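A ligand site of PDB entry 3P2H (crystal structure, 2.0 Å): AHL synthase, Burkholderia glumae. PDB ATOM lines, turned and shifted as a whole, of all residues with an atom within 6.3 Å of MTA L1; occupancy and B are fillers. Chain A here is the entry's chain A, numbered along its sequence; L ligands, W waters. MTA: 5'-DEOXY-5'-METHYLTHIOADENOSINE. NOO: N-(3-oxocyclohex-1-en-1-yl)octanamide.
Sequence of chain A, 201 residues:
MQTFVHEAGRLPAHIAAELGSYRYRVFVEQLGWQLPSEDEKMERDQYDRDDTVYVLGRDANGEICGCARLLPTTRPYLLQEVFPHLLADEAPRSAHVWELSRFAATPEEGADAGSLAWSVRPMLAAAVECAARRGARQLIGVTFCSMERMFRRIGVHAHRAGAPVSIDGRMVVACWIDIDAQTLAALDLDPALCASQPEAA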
ATOM      1  N   TRP A  33      10.546  24.635   0.760  1.00  0.00           N
ATOM      2  CA  TRP A  33      10.332  24.107   2.106  1.00  0.00           C
ATOM      3  C   TRP A  33      11.591  24.128   2.977  1.00  0.00           C
ATOM      4  O   TRP A  33      11.509  24.054   4.193  1.00  0.00           O
ATOM      5  CB  TRP A  33       9.783  22.682   2.051  1.00  0.00           C
ATOM      6  CG  TRP A  33       8.345  22.583   1.621  1.00  0.00           C
ATOM      7  CD1 TRP A  33       7.540  23.608   1.218  1.00  0.00           C
ATOM      8  CD2 TRP A  33       7.539  21.394   1.525  1.00  0.00           C
ATOM      9  NE1 TRP A  33       6.290  23.132   0.887  1.00  0.00           N
ATOM     10  CE2 TRP A  33       6.263  21.777   1.059  1.00  0.00           C
ATOM     11  CE3 TRP A  33       7.791  20.031   1.786  1.00  0.00           C
ATOM     12  CZ2 TRP A  33       5.234  20.853   0.850  1.00  0.00           C
ATOM     13  CZ3 TRP A  33       6.750  19.110   1.571  1.00  0.00           C
ATOM     14  CH2 TRP A  33       5.497  19.529   1.113  1.00  0.00           C
ATOM     15  N   GLN A  34      12.748  24.216   2.329  1.00  0.00           N
ATOM     16  CA  GLN A  34      14.030  24.243   3.032  1.00  0.00           C
ATOM     17  C   GLN A  34      14.996  25.186   2.323  1.00  0.00           C
ATOM     18  O   GLN A  34      14.736  25.619   1.190  1.00  0.00           O
ATOM     19  CB  GLN A  34      14.627  22.830   3.090  1.00  0.00           C
ATOM     20  CG  GLN A  34      13.737  21.805   3.809  1.00  0.00           C
ATOM     21  CD  GLN A  34      14.195  20.364   3.610  1.00  0.00           C
ATOM     22  OE1 GLN A  34      13.516  19.418   4.026  1.00  0.00           O
ATOM     23  NE2 GLN A  34      15.345  20.195   2.964  1.00  0.00           N
ATOM     24  N   GLU A  43      15.919  15.228  -1.105  1.00  0.00           N
ATOM     25  CA  GLU A  43      14.895  15.666  -0.156  1.00  0.00           C
ATOM     26  C   GLU A  43      14.262  14.402   0.410  1.00  0.00           C
ATOM     27  O   GLU A  43      13.576  13.685  -0.304  1.00  0.00           O
ATOM     28  CB  GLU A  43      13.835  16.520  -0.852  1.00  0.00           C
ATOM     29  CG  GLU A  43      12.763  17.091   0.077  1.00  0.00           C
ATOM     30  CD  GLU A  43      11.784  16.040   0.603  1.00  0.00           C
ATOM     31  OE1 GLU A  43      10.956  15.545  -0.181  1.00  0.00           O
ATOM     32  OE2 GLU A  43      11.850  15.712   1.805  1.00  0.00           O
ATOM     33  N   ASP A  45      12.848  12.591   4.485  1.00  0.00           N
ATOM     34  CA  ASP A  45      12.634  12.764   5.921  1.00  0.00           C
ATOM     35  C   ASP A  45      12.549  11.411   6.624  1.00  0.00           C
ATOM     36  O   ASP A  45      12.878  10.380   6.042  1.00  0.00           O
ATOM     37  CB  ASP A  45      11.358  13.577   6.192  1.00  0.00           C
ATOM     38  CG  ASP A  45      10.120  12.911   5.639  1.00  0.00           C
ATOM     39  OD1 ASP A  45      10.149  11.703   5.367  1.00  0.00           O
ATOM     40  OD2 ASP A  45       9.088  13.609   5.498  1.00  0.00           O
ATOM     41  N   GLN A  46      12.095  11.423   7.879  1.00  0.00           N
ATOM     42  CA  GLN A  46      11.992  10.195   8.667  1.00  0.00           C
ATOM     43  C   GLN A  46      10.915   9.229   8.167  1.00  0.00           C
ATOM     44  O   GLN A  46      10.850   8.083   8.627  1.00  0.00           O
ATOM     45  CB  GLN A  46      11.712  10.520  10.135  1.00  0.00           C
ATOM     46  CG  GLN A  46      10.325  11.077  10.408  1.00  0.00           C
ATOM     47  CD  GLN A  46      10.305  12.591  10.459  1.00  0.00           C
ATOM     48  OE1 GLN A  46      10.730  13.253   9.515  1.00  0.00           O
ATOM     49  NE2 GLN A  46       9.789  13.150  11.560  1.00  0.00           N
ATOM     50  N   TYR A  47      10.079   9.679   7.245  1.00  0.00           N
ATOM     51  CA  TYR A  47       9.020   8.827   6.725  1.00  0.00           C
ATOM     52  C   TYR A  47       9.403   8.041   5.469  1.00  0.00           C
ATOM     53  O   TYR A  47       8.587   7.291   4.928  1.00  0.00           O
ATOM     54  CB  TYR A  47       7.767   9.674   6.495  1.00  0.00           C
ATOM     55  CG  TYR A  47       7.336  10.310   7.793  1.00  0.00           C
ATOM     56  CD1 TYR A  47       6.846   9.525   8.835  1.00  0.00           C
ATOM     57  CD2 TYR A  47       7.524  11.669   8.028  1.00  0.00           C
ATOM     58  CE1 TYR A  47       6.565  10.074  10.083  1.00  0.00           C
ATOM     59  CE2 TYR A  47       7.250  12.227   9.267  1.00  0.00           C
ATOM     60  CZ  TYR A  47       6.781  11.424  10.286  1.00  0.00           C
ATOM     61  OH  TYR A  47       6.561  11.946  11.541  1.00  0.00           O
ATOM     62  N   ARG A  69       3.921   9.431  -2.079  1.00  0.00           N
ATOM     63  CA  ARG A  69       4.386   8.575  -1.003  1.00  0.00           C
ATOM     64  C   ARG A  69       3.169   8.004  -0.277  1.00  0.00           C
ATOM     65  O   ARG A  69       2.242   8.745   0.029  1.00  0.00           O
ATOM     66  CB  ARG A  69       5.261   9.377  -0.030  1.00  0.00           C
ATOM     67  CG  ARG A  69       5.786   8.584   1.132  1.00  0.00           C
ATOM     68  CD  ARG A  69       6.941   9.294   1.822  1.00  0.00           C
ATOM     69  NE  ARG A  69       6.510  10.427   2.639  1.00  0.00           N
ATOM     70  CZ  ARG A  69       7.342  11.203   3.319  1.00  0.00           C
ATOM     71  NH1 ARG A  69       8.641  10.971   3.274  1.00  0.00           N
ATOM     72  NH2 ARG A  69       6.875  12.191   4.068  1.00  0.00           N
ATOM     73  N   LEU A  78       3.432  11.298   8.836  1.00  0.00           N
ATOM     74  CA  LEU A  78       3.544  12.753   8.894  1.00  0.00           C
ATOM     75  C   LEU A  78       2.440  13.546   9.601  1.00  0.00           C
ATOM     76  O   LEU A  78       2.713  14.302  10.536  1.00  0.00           O
ATOM     77  CB  LEU A  78       3.773  13.296   7.473  1.00  0.00           C
ATOM     78  CG  LEU A  78       4.168  14.764   7.297  1.00  0.00           C
ATOM     79  CD1 LEU A  78       5.339  15.100   8.196  1.00  0.00           C
ATOM     80  CD2 LEU A  78       4.529  15.010   5.832  1.00  0.00           C
ATOM     81  N   VAL A  82       3.751  15.016  13.042  1.00  0.00           N
ATOM     82  CA  VAL A  82       4.129  16.397  12.825  1.00  0.00           C
ATOM     83  C   VAL A  82       2.989  17.412  12.844  1.00  0.00           C
ATOM     84  O   VAL A  82       3.105  18.463  13.489  1.00  0.00           O
ATOM     85  CB  VAL A  82       4.899  16.525  11.484  1.00  0.00           C
ATOM     86  CG1 VAL A  82       5.318  17.974  11.241  1.00  0.00           C
ATOM     87  CG2 VAL A  82       6.122  15.624  11.515  1.00  0.00           C
ATOM     88  N   PHE A  83       1.884  17.119  12.161  1.00  0.00           N
ATOM     89  CA  PHE A  83       0.765  18.055  12.119  1.00  0.00           C
ATOM     90  C   PHE A  83      -0.552  17.523  12.684  1.00  0.00           C
ATOM     91  O   PHE A  83      -1.609  17.702  12.083  1.00  0.00           O
ATOM     92  CB  PHE A  83       0.555  18.501  10.676  1.00  0.00           C
ATOM     93  CG  PHE A  83       1.740  19.193  10.080  1.00  0.00           C
ATOM     94  CD1 PHE A  83       2.190  20.409  10.598  1.00  0.00           C
ATOM     95  CD2 PHE A  83       2.414  18.640   8.991  1.00  0.00           C
ATOM     96  CE1 PHE A  83       3.297  21.068  10.044  1.00  0.00           C
ATOM     97  CE2 PHE A  83       3.513  19.290   8.432  1.00  0.00           C
ATOM     98  CZ  PHE A  83       3.953  20.510   8.958  1.00  0.00           C
ATOM     99  N   ARG A 102       3.901  13.837   0.037  1.00  0.00           N
ATOM    100  CA  ARG A 102       4.855  14.160  -1.018  1.00  0.00           C
ATOM    101  C   ARG A 102       4.237  13.848  -2.386  1.00  0.00           C
ATOM    102  O   ARG A 102       4.791  13.101  -3.182  1.00  0.00           O
ATOM    103  CB  ARG A 102       6.160  13.369  -0.829  1.00  0.00           C
ATOM    104  CG  ARG A 102       6.967  13.755   0.406  1.00  0.00           C
ATOM    105  CD  ARG A 102       7.406  15.220   0.373  1.00  0.00           C
ATOM    106  NE  ARG A 102       8.453  15.518   1.344  1.00  0.00           N
ATOM    107  CZ  ARG A 102       8.265  15.597   2.662  1.00  0.00           C
ATOM    108  NH1 ARG A 102       9.292  15.867   3.466  1.00  0.00           N
ATOM    109  NH2 ARG A 102       7.061  15.417   3.195  1.00  0.00           N
ATOM    110  N   VAL A 142      -2.194  15.842   4.412  1.00  0.00           N
ATOM    111  CA  VAL A 142      -2.231  17.293   4.320  1.00  0.00           C
ATOM    112  C   VAL A 142      -2.065  17.649   2.860  1.00  0.00           C
ATOM    113  O   VAL A 142      -1.101  17.231   2.213  1.00  0.00           O
ATOM    114  CB  VAL A 142      -1.091  17.939   5.140  1.00  0.00           C
ATOM    115  CG1 VAL A 142      -1.149  19.442   5.003  1.00  0.00           C
ATOM    116  CG2 VAL A 142      -1.203  17.524   6.583  1.00  0.00           C
ATOM    117  N   THR A 143      -3.002  18.420   2.333  1.00  0.00           N
ATOM    118  CA  THR A 143      -2.933  18.789   0.936  1.00  0.00           C
ATOM    119  C   THR A 143      -3.133  20.280   0.749  1.00  0.00           C
ATOM    120  O   THR A 143      -3.899  20.908   1.472  1.00  0.00           O
ATOM    121  CB  THR A 143      -4.033  18.066   0.117  1.00  0.00           C
ATOM    122  OG1 THR A 143      -5.163  18.928  -0.038  1.00  0.00           O
ATOM    123  CG2 THR A 143      -4.490  16.827   0.843  1.00  0.00           C
ATOM    124  N   PHE A 144      -2.418  20.851  -0.221  1.00  0.00           N
ATOM    125  CA  PHE A 144      -2.555  22.273  -0.518  1.00  0.00           C
ATOM    126  C   PHE A 144      -4.013  22.402  -0.964  1.00  0.00           C
ATOM    127  O   PHE A 144      -4.544  21.495  -1.612  1.00  0.00           O
ATOM    128  CB  PHE A 144      -1.633  22.655  -1.673  1.00  0.00           C
ATOM    129  CG  PHE A 144      -0.165  22.634  -1.316  1.00  0.00           C
ATOM    130  CD1 PHE A 144       0.297  21.932  -0.204  1.00  0.00           C
ATOM    131  CD2 PHE A 144       0.757  23.275  -2.129  1.00  0.00           C
ATOM    132  CE1 PHE A 144       1.666  21.889   0.091  1.00  0.00           C
ATOM    133  CE2 PHE A 144       2.123  23.238  -1.842  1.00  0.00           C
ATOM    134  CZ  PHE A 144       2.573  22.540  -0.735  1.00  0.00           C
ATOM    135  N   ILE A 167       0.021  27.659   6.273  1.00  0.00           N
ATOM    136  CA  ILE A 167       1.298  27.380   6.909  1.00  0.00           C
ATOM    137  C   ILE A 167       2.434  28.029   6.130  1.00  0.00           C
ATOM    138  O   ILE A 167       2.705  27.666   4.990  1.00  0.00           O
ATOM    139  CB  ILE A 167       1.553  25.871   7.018  1.00  0.00           C
ATOM    140  CG1 ILE A 167       0.440  25.209   7.845  1.00  0.00           C
ATOM    141  CG2 ILE A 167       2.909  25.613   7.655  1.00  0.00           C
ATOM    142  CD1 ILE A 167       0.498  23.708   7.859  1.00  0.00           C
ATOM    143  N   ASP A 168       3.107  28.988   6.767  1.00  0.00           N
ATOM    144  CA  ASP A 168       4.207  29.708   6.145  1.00  0.00           C
ATOM    145  C   ASP A 168       3.722  30.284   4.824  1.00  0.00           C
ATOM    146  O   ASP A 168       4.423  30.203   3.812  1.00  0.00           O
ATOM    147  CB  ASP A 168       5.402  28.793   5.916  1.00  0.00           C
ATOM    148  CG  ASP A 168       6.125  28.448   7.204  1.00  0.00           C
ATOM    149  OD1 ASP A 168       6.926  27.497   7.193  1.00  0.00           O
ATOM    150  OD2 ASP A 168       5.883  29.143   8.218  1.00  0.00           O
ATOM    151  N   ARG A 170       1.210  29.188   2.922  1.00  0.00           N
ATOM    152  CA  ARG A 170       0.579  28.241   1.991  1.00  0.00           C
ATOM    153  C   ARG A 170      -0.690  27.620   2.571  1.00  0.00           C
ATOM    154  O   ARG A 170      -0.640  26.897   3.566  1.00  0.00           O
ATOM    155  CB  ARG A 170       1.552  27.121   1.618  1.00  0.00           C
ATOM    156  CG  ARG A 170       2.689  27.550   0.693  1.00  0.00           C
ATOM    157  CD  ARG A 170       3.559  26.357   0.284  1.00  0.00           C
ATOM    158  NE  ARG A 170       4.526  25.999   1.315  1.00  0.00           N
ATOM    159  CZ  ARG A 170       5.462  26.837   1.775  1.00  0.00           C
ATOM    160  NH1 ARG A 170       5.551  28.068   1.282  1.00  0.00           N
ATOM    161  NH2 ARG A 170       6.309  26.443   2.727  1.00  0.00           N
ATOM    162  N   VAL A 172      -3.398  25.124   3.278  1.00  0.00           N
ATOM    163  CA  VAL A 172      -3.488  23.668   3.224  1.00  0.00           C
ATOM    164  C   VAL A 172      -4.614  23.182   4.124  1.00  0.00           C
ATOM    165  O   VAL A 172      -5.178  23.934   4.929  1.00  0.00           O
ATOM    166  CB  VAL A 172      -2.180  22.993   3.675  1.00  0.00           C
ATOM    167  CG1 VAL A 172      -0.998  23.552   2.911  1.00  0.00           C
ATOM    168  CG2 VAL A 172      -1.991  23.189   5.180  1.00  0.00           C
HETATM  169  CS  MTA L   1       2.928  19.163   4.032  1.00  0.00           C
HETATM  170  S5' MTA L   1       2.588  20.894   4.447  1.00  0.00           S
HETATM  171  C5' MTA L   1       4.180  21.676   4.042  1.00  0.00           C
HETATM  172  C4' MTA L   1       5.068  21.864   5.267  1.00  0.00           C
HETATM  173  O4' MTA L   1       5.346  20.543   5.815  1.00  0.00           O
HETATM  174  C2' MTA L   1       7.424  21.384   5.149  1.00  0.00           C
HETATM  175  O2' MTA L   1       8.746  21.849   5.456  1.00  0.00           O
HETATM  176  C3' MTA L   1       6.388  22.513   4.842  1.00  0.00           C
HETATM  177  O3' MTA L   1       6.651  23.642   5.674  1.00  0.00           O
HETATM  178  C1' MTA L   1       6.728  20.591   6.264  1.00  0.00           C
HETATM  179  N9  MTA L   1       7.233  19.208   6.383  1.00  0.00           N
HETATM  180  C8  MTA L   1       7.213  18.225   5.417  1.00  0.00           C
HETATM  181  N7  MTA L   1       7.730  17.124   5.854  1.00  0.00           N
HETATM  182  C5  MTA L   1       8.137  17.310   7.142  1.00  0.00           C
HETATM  183  C6  MTA L   1       8.765  16.500   8.140  1.00  0.00           C
HETATM  184  N6  MTA L   1       9.091  15.181   7.849  1.00  0.00           N
HETATM  185  N1  MTA L   1       9.019  17.039   9.376  1.00  0.00           N
HETATM  186  C2  MTA L   1       8.702  18.331   9.682  1.00  0.00           C
HETATM  187  N3  MTA L   1       8.109  19.116   8.732  1.00  0.00           N
HETATM  188  C4  MTA L   1       7.810  18.668   7.494  1.00  0.00           C
HETATM  189  C1  NOO L   2       1.302  20.523  -4.794  1.00  0.00           C
HETATM  190  O1  NOO L   2       0.535  21.341  -5.292  1.00  0.00           O
HETATM  191  C2  NOO L   2       0.851  19.498  -3.765  1.00  0.00           C
HETATM  192  C3  NOO L   2       1.710  19.008  -2.763  1.00  0.00           C
HETATM  193  C4  NOO L   2       3.208  19.367  -2.888  1.00  0.00           C
HETATM  194  C5  NOO L   2       3.721  19.587  -4.365  1.00  0.00           C
HETATM  195  C6  NOO L   2       2.811  20.534  -5.205  1.00  0.00           C
HETATM  196  N7  NOO L   2       1.306  18.191  -1.630  1.00  0.00           N
HETATM  197  C8  NOO L   2       1.819  17.025  -1.001  1.00  0.00           C
HETATM  198  O8  NOO L   2       2.984  16.895  -0.620  1.00  0.00           O
HETATM  199  C9  NOO L   2       0.887  15.827  -0.741  1.00  0.00           C
HETATM  200  C10 NOO L   2      -0.646  15.987  -0.900  1.00  0.00           C
HETATM  201  C11 NOO L   2      -1.368  14.981   0.044  1.00  0.00           C
HETATM  202  C12 NOO L   2      -2.623  14.364  -0.596  1.00  0.00           C
HETATM  203  C13 NOO L   2      -3.385  13.475   0.408  1.00  0.00           C
HETATM  204  C14 NOO L   2      -4.908  13.486   0.146  1.00  0.00           C
HETATM  205  C15 NOO L   2      -5.635  12.437   0.987  1.00  0.00           C
HETATM  206  O   HOH W   1      10.010  16.143  11.598  1.00  0.00           O
HETATM  207  O   HOH W   2      10.951  19.792   4.478  1.00  0.00           O
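NH1 of Arg 102 sits at hydrogen-bond distance from N7 of MTA L1. OE1 of Gln 46 is in hydrogen-bond range of N6 of MTA L1 (3.0 Å). The side-chain carboxylate of Asp 45 lies within hydrogen-bond range of a nitrogen (N6) of MTA L1, at 2.8 Å. An oxygen (O8) of NOO L2 sits at hydrogen-bond distance from the backbone NH (N) of Arg 102, at 3.3 Å.
The backbone carbonyl oxygen (O) of Leu 78 is in hydrogen-bond range of the backbone NH (N) of Phe 83 (3.4 Å). The side-chain carboxylate (OE1) of Glu 43 lies within salt-bridge range of the guanidinium group (NE) of Arg 102, 2.9 Å away. The backbone NH of Tyr 47 is in hydrogen-bond range of the side-chain carboxylate of Asp 45 (2.8 Å). The side-chain amide nitrogen (NE2) of Gln 46 is in hydrogen-bond range of the side-chain hydroxyl (OH) of Tyr 47, at 3.4 Å. The side-chain carboxylate (OD1) of Asp 45 is in salt-bridge range of the guanidinium group (NH1) of Arg 69, 2.7 Å away. The side-chain carboxylate (OD2) of Asp 45 lies within salt-bridge range of the guanidinium group (NH1) of Arg 102 (3.0 Å).
Residues that only touch MTA L1: Trp 33 (3.5 Å), Tyr 47 (3.8 Å), Leu 78 (3.7 Å), Val 82 (3.7 Å) and Phe 83 (3.4 Å). Hydrophobic or aromatic side chains that line MTA L1: Trp 33, Tyr 47, Leu 78, Val 82 and Phe 83. Of the 18 residues printed, 8 come within 4 Å of MTA L1. Along chain A the residues within 4 Å of MTA L1 span positions 33 to 102.
Water W1 bridges N1 of MTA L1 (2.6 Å) and NE2 of Gln 46 (3.0 Å). Water W2 bridges OE1 of Gln 34 (2.6 Å) and O2' of MTA L1 (3.2 Å).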
